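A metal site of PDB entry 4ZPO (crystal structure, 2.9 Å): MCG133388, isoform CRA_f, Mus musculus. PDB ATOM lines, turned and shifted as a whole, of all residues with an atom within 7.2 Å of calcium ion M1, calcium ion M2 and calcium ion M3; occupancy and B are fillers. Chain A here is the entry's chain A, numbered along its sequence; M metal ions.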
ATOM      1  N   GLU A   8     -12.861   9.680 -37.336  1.00  0.00           N
ATOM      2  CA  GLU A   8     -12.773   8.219 -37.390  1.00  0.00           C
ATOM      3  C   GLU A   8     -13.795   7.653 -38.368  1.00  0.00           C
ATOM      4  O   GLU A   8     -14.853   8.251 -38.589  1.00  0.00           O
ATOM      5  CB  GLU A   8     -12.994   7.641 -35.988  1.00  0.00           C
ATOM      6  CG  GLU A   8     -12.893   6.131 -35.892  1.00  0.00           C
ATOM      7  CD  GLU A   8     -13.671   5.580 -34.714  1.00  0.00           C
ATOM      8  OE1 GLU A   8     -14.195   6.384 -33.919  1.00  0.00           O
ATOM      9  OE2 GLU A   8     -13.781   4.339 -34.600  1.00  0.00           O
ATOM     10  N   GLU A   9     -13.460   6.509 -38.974  1.00  0.00           N
ATOM     11  CA  GLU A   9     -14.352   5.782 -39.885  1.00  0.00           C
ATOM     12  C   GLU A   9     -14.681   6.569 -41.157  1.00  0.00           C
ATOM     13  O   GLU A   9     -15.645   6.257 -41.855  1.00  0.00           O
ATOM     14  CB  GLU A   9     -15.655   5.402 -39.178  1.00  0.00           C
ATOM     15  CG  GLU A   9     -15.477   4.697 -37.849  1.00  0.00           C
ATOM     16  CD  GLU A   9     -14.903   3.304 -37.990  1.00  0.00           C
ATOM     17  OE1 GLU A   9     -14.918   2.755 -39.116  1.00  0.00           O
ATOM     18  OE2 GLU A   9     -14.425   2.750 -36.978  1.00  0.00           O
ATOM     19  N   ILE A  61      -9.923   4.207 -40.948  1.00  0.00           N
ATOM     20  CA  ILE A  61      -9.256   4.205 -39.655  1.00  0.00           C
ATOM     21  C   ILE A  61     -10.217   3.923 -38.505  1.00  0.00           C
ATOM     22  O   ILE A  61     -11.241   4.594 -38.363  1.00  0.00           O
ATOM     23  CB  ILE A  61      -8.540   5.542 -39.378  1.00  0.00           C
ATOM     24  CG1 ILE A  61      -7.454   5.786 -40.433  1.00  0.00           C
ATOM     25  CG2 ILE A  61      -7.949   5.568 -37.980  1.00  0.00           C
ATOM     26  CD1 ILE A  61      -6.771   7.126 -40.304  1.00  0.00           C
ATOM     27  N   ASP A  62      -9.876   2.941 -37.674  1.00  0.00           N
ATOM     28  CA  ASP A  62     -10.664   2.634 -36.481  1.00  0.00           C
ATOM     29  C   ASP A  62      -9.940   3.150 -35.245  1.00  0.00           C
ATOM     30  O   ASP A  62      -8.887   2.641 -34.875  1.00  0.00           O
ATOM     31  CB  ASP A  62     -10.906   1.119 -36.372  1.00  0.00           C
ATOM     32  CG  ASP A  62     -11.864   0.773 -35.251  1.00  0.00           C
ATOM     33  OD1 ASP A  62     -12.711   1.614 -34.899  1.00  0.00           O
ATOM     34  OD2 ASP A  62     -11.758  -0.349 -34.717  1.00  0.00           O
ATOM     35  N   ARG A  63     -10.524   4.156 -34.604  1.00  0.00           N
ATOM     36  CA  ARG A  63      -9.883   4.795 -33.456  1.00  0.00           C
ATOM     37  C   ARG A  63      -9.767   3.851 -32.265  1.00  0.00           C
ATOM     38  O   ARG A  63      -8.824   3.942 -31.473  1.00  0.00           O
ATOM     39  CB  ARG A  63     -10.655   6.049 -33.035  1.00  0.00           C
ATOM     40  CG  ARG A  63      -9.901   6.940 -32.071  1.00  0.00           C
ATOM     41  CD  ARG A  63     -10.837   7.589 -31.062  1.00  0.00           C
ATOM     42  NE  ARG A  63     -11.518   6.579 -30.250  1.00  0.00           N
ATOM     43  CZ  ARG A  63     -11.027   6.084 -29.117  1.00  0.00           C
ATOM     44  NH1 ARG A  63     -11.707   5.166 -28.451  1.00  0.00           N
ATOM     45  NH2 ARG A  63      -9.850   6.502 -28.662  1.00  0.00           N
ATOM     46  N   GLU A  64     -10.723   2.941 -32.142  1.00  0.00           N
ATOM     47  CA  GLU A  64     -10.722   1.974 -31.041  1.00  0.00           C
ATOM     48  C   GLU A  64      -9.596   0.958 -31.174  1.00  0.00           C
ATOM     49  O   GLU A  64      -9.099   0.424 -30.179  1.00  0.00           O
ATOM     50  CB  GLU A  64     -12.063   1.250 -30.954  1.00  0.00           C
ATOM     51  CG  GLU A  64     -13.156   2.024 -30.216  1.00  0.00           C
ATOM     52  CD  GLU A  64     -13.576   3.290 -30.930  1.00  0.00           C
ATOM     53  OE1 GLU A  64     -13.420   4.382 -30.357  1.00  0.00           O
ATOM     54  OE2 GLU A  64     -14.071   3.176 -32.075  1.00  0.00           O
ATOM     55  N   SER A  65      -9.184   0.691 -32.412  1.00  0.00           N
ATOM     56  CA  SER A  65      -8.146  -0.290 -32.681  1.00  0.00           C
ATOM     57  C   SER A  65      -6.745   0.274 -32.483  1.00  0.00           C
ATOM     58  O   SER A  65      -5.800  -0.461 -32.186  1.00  0.00           O
ATOM     59  CB  SER A  65      -8.284  -0.842 -34.098  1.00  0.00           C
ATOM     60  OG  SER A  65      -9.509  -1.546 -34.252  1.00  0.00           O
ATOM     61  N   LEU A  95     -10.335  11.967 -34.299  1.00  0.00           N
ATOM     62  CA  LEU A  95     -11.514  12.330 -33.527  1.00  0.00           C
ATOM     63  C   LEU A  95     -12.425  11.125 -33.307  1.00  0.00           C
ATOM     64  O   LEU A  95     -12.686  10.358 -34.230  1.00  0.00           O
ATOM     65  CB  LEU A  95     -12.281  13.456 -34.230  1.00  0.00           C
ATOM     66  CG  LEU A  95     -11.480  14.718 -34.538  1.00  0.00           C
ATOM     67  CD1 LEU A  95     -12.356  15.759 -35.218  1.00  0.00           C
ATOM     68  CD2 LEU A  95     -10.847  15.286 -33.280  1.00  0.00           C
ATOM     69  N   ASP A  96     -12.902  10.970 -32.080  1.00  0.00           N
ATOM     70  CA  ASP A  96     -13.717   9.816 -31.718  1.00  0.00           C
ATOM     71  C   ASP A  96     -15.137   9.921 -32.261  1.00  0.00           C
ATOM     72  O   ASP A  96     -15.774  10.974 -32.200  1.00  0.00           O
ATOM     73  CB  ASP A  96     -13.768   9.652 -30.198  1.00  0.00           C
ATOM     74  CG  ASP A  96     -14.650   8.500 -29.765  1.00  0.00           C
ATOM     75  OD1 ASP A  96     -14.687   7.473 -30.472  1.00  0.00           O
ATOM     76  OD2 ASP A  96     -15.321   8.614 -28.712  1.00  0.00           O
ATOM     77  N   LEU A  97     -15.636   8.808 -32.789  1.00  0.00           N
ATOM     78  CA  LEU A  97     -17.010   8.710 -33.258  1.00  0.00           C
ATOM     79  C   LEU A  97     -17.788   7.783 -32.333  1.00  0.00           C
ATOM     80  O   LEU A  97     -17.226   6.862 -31.747  1.00  0.00           O
ATOM     81  CB  LEU A  97     -17.045   8.188 -34.702  1.00  0.00           C
ATOM     82  CG  LEU A  97     -18.229   8.604 -35.576  1.00  0.00           C
ATOM     83  CD1 LEU A  97     -18.247  10.107 -35.774  1.00  0.00           C
ATOM     84  CD2 LEU A  97     -18.176   7.879 -36.912  1.00  0.00           C
ATOM     85  N   ASN A  98     -19.091   8.032 -32.193  1.00  0.00           N
ATOM     86  CA  ASN A  98     -19.915   7.200 -31.312  1.00  0.00           C
ATOM     87  C   ASN A  98     -20.554   6.049 -32.065  1.00  0.00           C
ATOM     88  O   ASN A  98     -21.779   5.995 -32.217  1.00  0.00           O
ATOM     89  CB  ASN A  98     -20.994   8.058 -30.644  1.00  0.00           C
ATOM     90  CG  ASN A  98     -21.713   7.318 -29.526  1.00  0.00           C
ATOM     91  OD1 ASN A  98     -21.119   6.493 -28.827  1.00  0.00           O
ATOM     92  ND2 ASN A  98     -22.996   7.604 -29.353  1.00  0.00           N
ATOM     93  N   ASP A  99     -19.727   5.120 -32.545  1.00  0.00           N
ATOM     94  CA  ASP A  99     -20.213   4.014 -33.360  1.00  0.00           C
ATOM     95  C   ASP A  99     -20.154   2.682 -32.622  1.00  0.00           C
ATOM     96  O   ASP A  99     -20.372   1.619 -33.218  1.00  0.00           O
ATOM     97  CB  ASP A  99     -19.412   3.929 -34.652  1.00  0.00           C
ATOM     98  CG  ASP A  99     -17.919   3.851 -34.419  1.00  0.00           C
ATOM     99  OD1 ASP A  99     -17.428   4.453 -33.436  1.00  0.00           O
ATOM    100  OD2 ASP A  99     -17.226   3.185 -35.219  1.00  0.00           O
ATOM    101  N   ASN A 100     -19.867   2.726 -31.321  1.00  0.00           N
ATOM    102  CA  ASN A 100     -19.854   1.516 -30.506  1.00  0.00           C
ATOM    103  C   ASN A 100     -20.988   1.509 -29.483  1.00  0.00           C
ATOM    104  O   ASN A 100     -21.298   2.535 -28.874  1.00  0.00           O
ATOM    105  CB  ASN A 100     -18.510   1.365 -29.786  1.00  0.00           C
ATOM    106  CG  ASN A 100     -17.435   0.795 -30.686  1.00  0.00           C
ATOM    107  OD1 ASN A 100     -17.255  -0.426 -30.755  1.00  0.00           O
ATOM    108  ND2 ASN A 100     -16.708   1.667 -31.378  1.00  0.00           N
ATOM    109  N   SER A 101     -21.606   0.352 -29.307  1.00  0.00           N
ATOM    110  CA  SER A 101     -22.741   0.210 -28.392  1.00  0.00           C
ATOM    111  C   SER A 101     -22.334  -0.528 -27.116  1.00  0.00           C
ATOM    112  O   SER A 101     -21.512  -1.449 -27.171  1.00  0.00           O
ATOM    113  CB  SER A 101     -23.894  -0.519 -29.075  1.00  0.00           C
ATOM    114  OG  SER A 101     -24.297   0.156 -30.255  1.00  0.00           O
ATOM    115  N   PRO A 102     -22.894  -0.111 -25.963  1.00  0.00           N
ATOM    116  CA  PRO A 102     -22.636  -0.725 -24.664  1.00  0.00           C
ATOM    117  C   PRO A 102     -22.792  -2.246 -24.681  1.00  0.00           C
ATOM    118  O   PRO A 102     -23.799  -2.766 -25.160  1.00  0.00           O
ATOM    119  CB  PRO A 102     -23.692  -0.085 -23.769  1.00  0.00           C
ATOM    120  CG  PRO A 102     -23.883   1.266 -24.356  1.00  0.00           C
ATOM    121  CD  PRO A 102     -23.755   1.078 -25.849  1.00  0.00           C
ATOM    122  N   GLN A 129     -19.598  -2.345 -21.045  1.00  0.00           N
ATOM    123  CA  GLN A 129     -18.403  -1.773 -21.649  1.00  0.00           C
ATOM    124  C   GLN A 129     -18.736  -0.980 -22.908  1.00  0.00           C
ATOM    125  O   GLN A 129     -19.625  -1.362 -23.677  1.00  0.00           O
ATOM    126  CB  GLN A 129     -17.388  -2.867 -21.977  1.00  0.00           C
ATOM    127  CG  GLN A 129     -16.956  -3.691 -20.779  1.00  0.00           C
ATOM    128  CD  GLN A 129     -16.174  -4.922 -21.181  1.00  0.00           C
ATOM    129  OE1 GLN A 129     -15.882  -5.123 -22.359  1.00  0.00           O
ATOM    130  NE2 GLN A 129     -15.841  -5.750 -20.212  1.00  0.00           N
ATOM    131  N   ASP A 130     -18.009   0.111 -23.124  1.00  0.00           N
ATOM    132  CA  ASP A 130     -18.160   0.926 -24.323  1.00  0.00           C
ATOM    133  C   ASP A 130     -16.795   1.488 -24.702  1.00  0.00           C
ATOM    134  O   ASP A 130     -16.334   2.461 -24.121  1.00  0.00           O
ATOM    135  CB  ASP A 130     -19.169   2.056 -24.082  1.00  0.00           C
ATOM    136  CG  ASP A 130     -19.691   2.665 -25.376  1.00  0.00           C
ATOM    137  OD1 ASP A 130     -18.958   2.648 -26.387  1.00  0.00           O
ATOM    138  OD2 ASP A 130     -20.837   3.160 -25.375  1.00  0.00           O
ATOM    139  N   PRO A 131     -16.155   0.872 -25.710  1.00  0.00           N
ATOM    140  CA  PRO A 131     -14.775   1.202 -26.107  1.00  0.00           C
ATOM    141  C   PRO A 131     -14.604   2.629 -26.630  1.00  0.00           C
ATOM    142  O   PRO A 131     -13.471   3.040 -26.868  1.00  0.00           O
ATOM    143  CB  PRO A 131     -14.481   0.187 -27.215  1.00  0.00           C
ATOM    144  CG  PRO A 131     -15.815  -0.203 -27.740  1.00  0.00           C
ATOM    145  CD  PRO A 131     -16.727  -0.188 -26.557  1.00  0.00           C
ATOM    146  N   ASP A 132     -15.697   3.364 -26.783  1.00  0.00           N
ATOM    147  CA  ASP A 132     -15.606   4.767 -27.190  1.00  0.00           C
ATOM    148  C   ASP A 132     -15.038   5.618 -26.065  1.00  0.00           C
ATOM    149  O   ASP A 132     -14.906   5.149 -24.931  1.00  0.00           O
ATOM    150  CB  ASP A 132     -16.975   5.287 -27.642  1.00  0.00           C
ATOM    151  CG  ASP A 132     -17.425   4.691 -28.958  1.00  0.00           C
ATOM    152  OD1 ASP A 132     -16.553   4.229 -29.735  1.00  0.00           O
ATOM    153  OD2 ASP A 132     -18.646   4.697 -29.241  1.00  0.00           O
ATOM    154  N   VAL A 133     -14.724   6.868 -26.369  1.00  0.00           N
ATOM    155  CA  VAL A 133     -14.001   7.723 -25.419  1.00  0.00           C
ATOM    156  C   VAL A 133     -14.689   9.061 -25.204  1.00  0.00           C
ATOM    157  O   VAL A 133     -15.164   9.701 -26.145  1.00  0.00           O
ATOM    158  CB  VAL A 133     -12.548   7.948 -25.904  1.00  0.00           C
ATOM    159  CG1 VAL A 133     -11.949   9.231 -25.324  1.00  0.00           C
ATOM    160  CG2 VAL A 133     -11.684   6.747 -25.557  1.00  0.00           C
ATOM    161  N   THR A 135     -17.660  11.338 -23.721  1.00  0.00           N
ATOM    162  CA  THR A 135     -19.070  11.204 -23.389  1.00  0.00           C
ATOM    163  C   THR A 135     -19.688  10.042 -24.145  1.00  0.00           C
ATOM    164  O   THR A 135     -20.758   9.554 -23.797  1.00  0.00           O
ATOM    165  CB  THR A 135     -19.852  12.498 -23.708  1.00  0.00           C
ATOM    166  OG1 THR A 135     -19.791  12.760 -25.117  1.00  0.00           O
ATOM    167  CG2 THR A 135     -19.263  13.684 -22.950  1.00  0.00           C
ATOM    168  N   ASN A 136     -18.985   9.573 -25.181  1.00  0.00           N
ATOM    169  CA  ASN A 136     -19.492   8.512 -26.033  1.00  0.00           C
ATOM    170  C   ASN A 136     -19.453   7.133 -25.375  1.00  0.00           C
ATOM    171  O   ASN A 136     -19.981   6.160 -25.926  1.00  0.00           O
ATOM    172  CB  ASN A 136     -18.705   8.476 -27.352  1.00  0.00           C
ATOM    173  CG  ASN A 136     -18.901   9.723 -28.185  1.00  0.00           C
ATOM    174  OD1 ASN A 136     -19.943  10.374 -28.108  1.00  0.00           O
ATOM    175  ND2 ASN A 136     -17.901  10.073 -28.984  1.00  0.00           N
ATOM    176  N   THR A 137     -18.829   7.045 -24.211  1.00  0.00           N
ATOM    177  CA  THR A 137     -18.797   5.788 -23.460  1.00  0.00           C
ATOM    178  C   THR A 137     -19.994   5.716 -22.518  1.00  0.00           C
ATOM    179  O   THR A 137     -20.793   6.652 -22.450  1.00  0.00           O
ATOM    180  CB  THR A 137     -17.489   5.640 -22.656  1.00  0.00           C
ATOM    181  OG1 THR A 137     -17.447   4.338 -22.055  1.00  0.00           O
ATOM    182  CG2 THR A 137     -17.406   6.697 -21.571  1.00  0.00           C
ATOM    183  N   VAL A 138     -20.108   4.601 -21.798  1.00  0.00           N
ATOM    184  CA  VAL A 138     -21.235   4.339 -20.894  1.00  0.00           C
ATOM    185  C   VAL A 138     -21.528   5.520 -19.963  1.00  0.00           C
ATOM    186  O   VAL A 138     -20.642   6.016 -19.278  1.00  0.00           O
ATOM    187  CB  VAL A 138     -20.975   3.083 -20.028  1.00  0.00           C
ATOM    188  CG1 VAL A 138     -22.082   2.901 -19.001  1.00  0.00           C
ATOM    189  CG2 VAL A 138     -20.852   1.855 -20.912  1.00  0.00           C
ATOM    190  N   ASP A 187     -24.970   5.001 -23.291  1.00  0.00           N
ATOM    191  CA  ASP A 187     -23.856   5.934 -23.374  1.00  0.00           C
ATOM    192  C   ASP A 187     -24.383   7.362 -23.493  1.00  0.00           C
ATOM    193  O   ASP A 187     -25.587   7.588 -23.492  1.00  0.00           O
ATOM    194  CB  ASP A 187     -22.929   5.595 -24.552  1.00  0.00           C
ATOM    195  CG  ASP A 187     -23.654   5.560 -25.896  1.00  0.00           C
ATOM    196  OD1 ASP A 187     -24.367   6.539 -26.232  1.00  0.00           O
ATOM    197  OD2 ASP A 187     -23.495   4.564 -26.624  1.00  0.00           O
ATOM    198  N   GLY A 188     -23.467   8.330 -23.592  1.00  0.00           N
ATOM    199  CA  GLY A 188     -23.846   9.726 -23.650  1.00  0.00           C
ATOM    200  C   GLY A 188     -23.582  10.365 -25.002  1.00  0.00           C
ATOM    201  O   GLY A 188     -23.002  11.449 -25.080  1.00  0.00           O
ATOM    202  N   GLY A 189     -23.991   9.696 -26.063  1.00  0.00           N
ATOM    203  CA  GLY A 189     -23.846  10.227 -27.411  1.00  0.00           C
ATOM    204  C   GLY A 189     -25.168  10.726 -27.958  1.00  0.00           C
ATOM    205  O   GLY A 189     -26.213  10.521 -27.357  1.00  0.00           O
ATOM    206  N   ARG A 193     -26.717   5.212 -27.664  1.00  0.00           N
ATOM    207  CA  ARG A 193     -26.763   3.799 -28.019  1.00  0.00           C
ATOM    208  C   ARG A 193     -26.792   2.957 -26.744  1.00  0.00           C
ATOM    209  O   ARG A 193     -26.219   3.352 -25.728  1.00  0.00           O
ATOM    210  CB  ARG A 193     -25.563   3.415 -28.880  1.00  0.00           C
ATOM    211  CG  ARG A 193     -25.173   4.509 -29.870  1.00  0.00           C
ATOM    212  CD  ARG A 193     -23.914   4.137 -30.636  1.00  0.00           C
ATOM    213  NE  ARG A 193     -24.193   3.250 -31.754  1.00  0.00           N
ATOM    214  CZ  ARG A 193     -24.318   3.664 -33.018  1.00  0.00           C
ATOM    215  NH1 ARG A 193     -24.169   4.936 -33.319  1.00  0.00           N
ATOM    216  NH2 ARG A 193     -24.568   2.778 -33.976  1.00  0.00           N
HETATM  217 CA    CA M   1     -20.608   4.437 -27.578  1.00  0.00          CA
HETATM  218 CA    CA M   2     -15.357   5.309 -31.771  1.00  0.00          CA
HETATM  219 CA    CA M   3     -14.968   2.255 -34.344  1.00  0.00          CA
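OE2 of Glu 64 lies close to ND2 of Asn 100. OG of Ser 65 sits at hydrogen-bond distance from OD2 of Asp 62 (2.6 Å). O of Asn 98 is in hydrogen-bond range of NH1 of Arg 193 (2.8 Å). OG1 of Thr 137 lies within hydrogen-bond range of O of Asp 130, at 3.0 Å. The side-chain carboxylate (OD1) of Asp 96 sits close to the guanidinium group (NE) of Arg 63 (3.3 Å). The backbone NH (N) of Val 133 sits at hydrogen-bond distance from the side-chain carboxylate (OD2) of Asp 96 (3.0 Å). O of Ile 61 lies within hydrogen-bond range of N of Glu 9, at 3.0 Å. OD1 of Asp 187 is in hydrogen-bond range of N of Gly 189 (3.2 Å).
Of the 28 residues printed, 6 come within 4 Å of calcium ion M1.
The nearest printed residue that does not touch calcium ion M2 is Arg 63 (4.3 Å).
Within 4 Å of calcium ion M3: Glu 8, Glu 9, Asp 62, Glu 64, Asp 99 and Asn 100. Along chain A the residues within 4 Å of calcium ion M3 span positions 8 to 100. The nearest printed residue that does not touch calcium ion M3 is Arg 63 (4.8 Å).
Calcium ion M1 is bound by the backbone carbonyl oxygen (O) of Asn 100, the side-chain amide oxygen (OD1) of Asn 98, the backbone carbonyl oxygen (O) of Asn 136, the side-chain carboxylate (OD2) of Asp 130, the side-chain carboxylate (OD2) of Asp 132 and the side-chain carboxylate (OD1) of Asp 130. Calcium ion M1 has six donor atoms within binding distance. Slightly farther from calcium ion M1 lies OD2 of Asp 187 (3.0 Å).
The backbone carbonyl oxygen (O) of Leu 97 binds calcium ion M2 (2.4 Å). OE2 of Glu 64 binds calcium ion M2, at 2.5 Å. OE1 of Glu 64 is bound to calcium ion M2, 2.6 Å away. The side-chain carboxylate (OD1) of Asp 132 binds calcium ion M2, 2.6 Å away. OD1 of Asp 96 is bound to calcium ion M2 (2.6 Å). OE1 of Glu 8 is bound to calcium ion M2 (2.7 Å). OD1 of Asp 99 binds calcium ion M2 (2.8 Å). Calcium ion M2 has seven donor atoms within binding distance.
Calcium ion M3 is bound by the side-chain carboxylate of Asp 62 (2.4 Å), the side-chain carboxylate of Glu 8 (2.4 Å), the side-chain carboxylate of Asp 99 (2.6 Å), the side-chain carboxylate of Glu 64 (2.6 Å) and the side-chain carboxylate of Glu 9 (2.7 Å). Calcium ion M3 has five donor atoms within binding distance.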
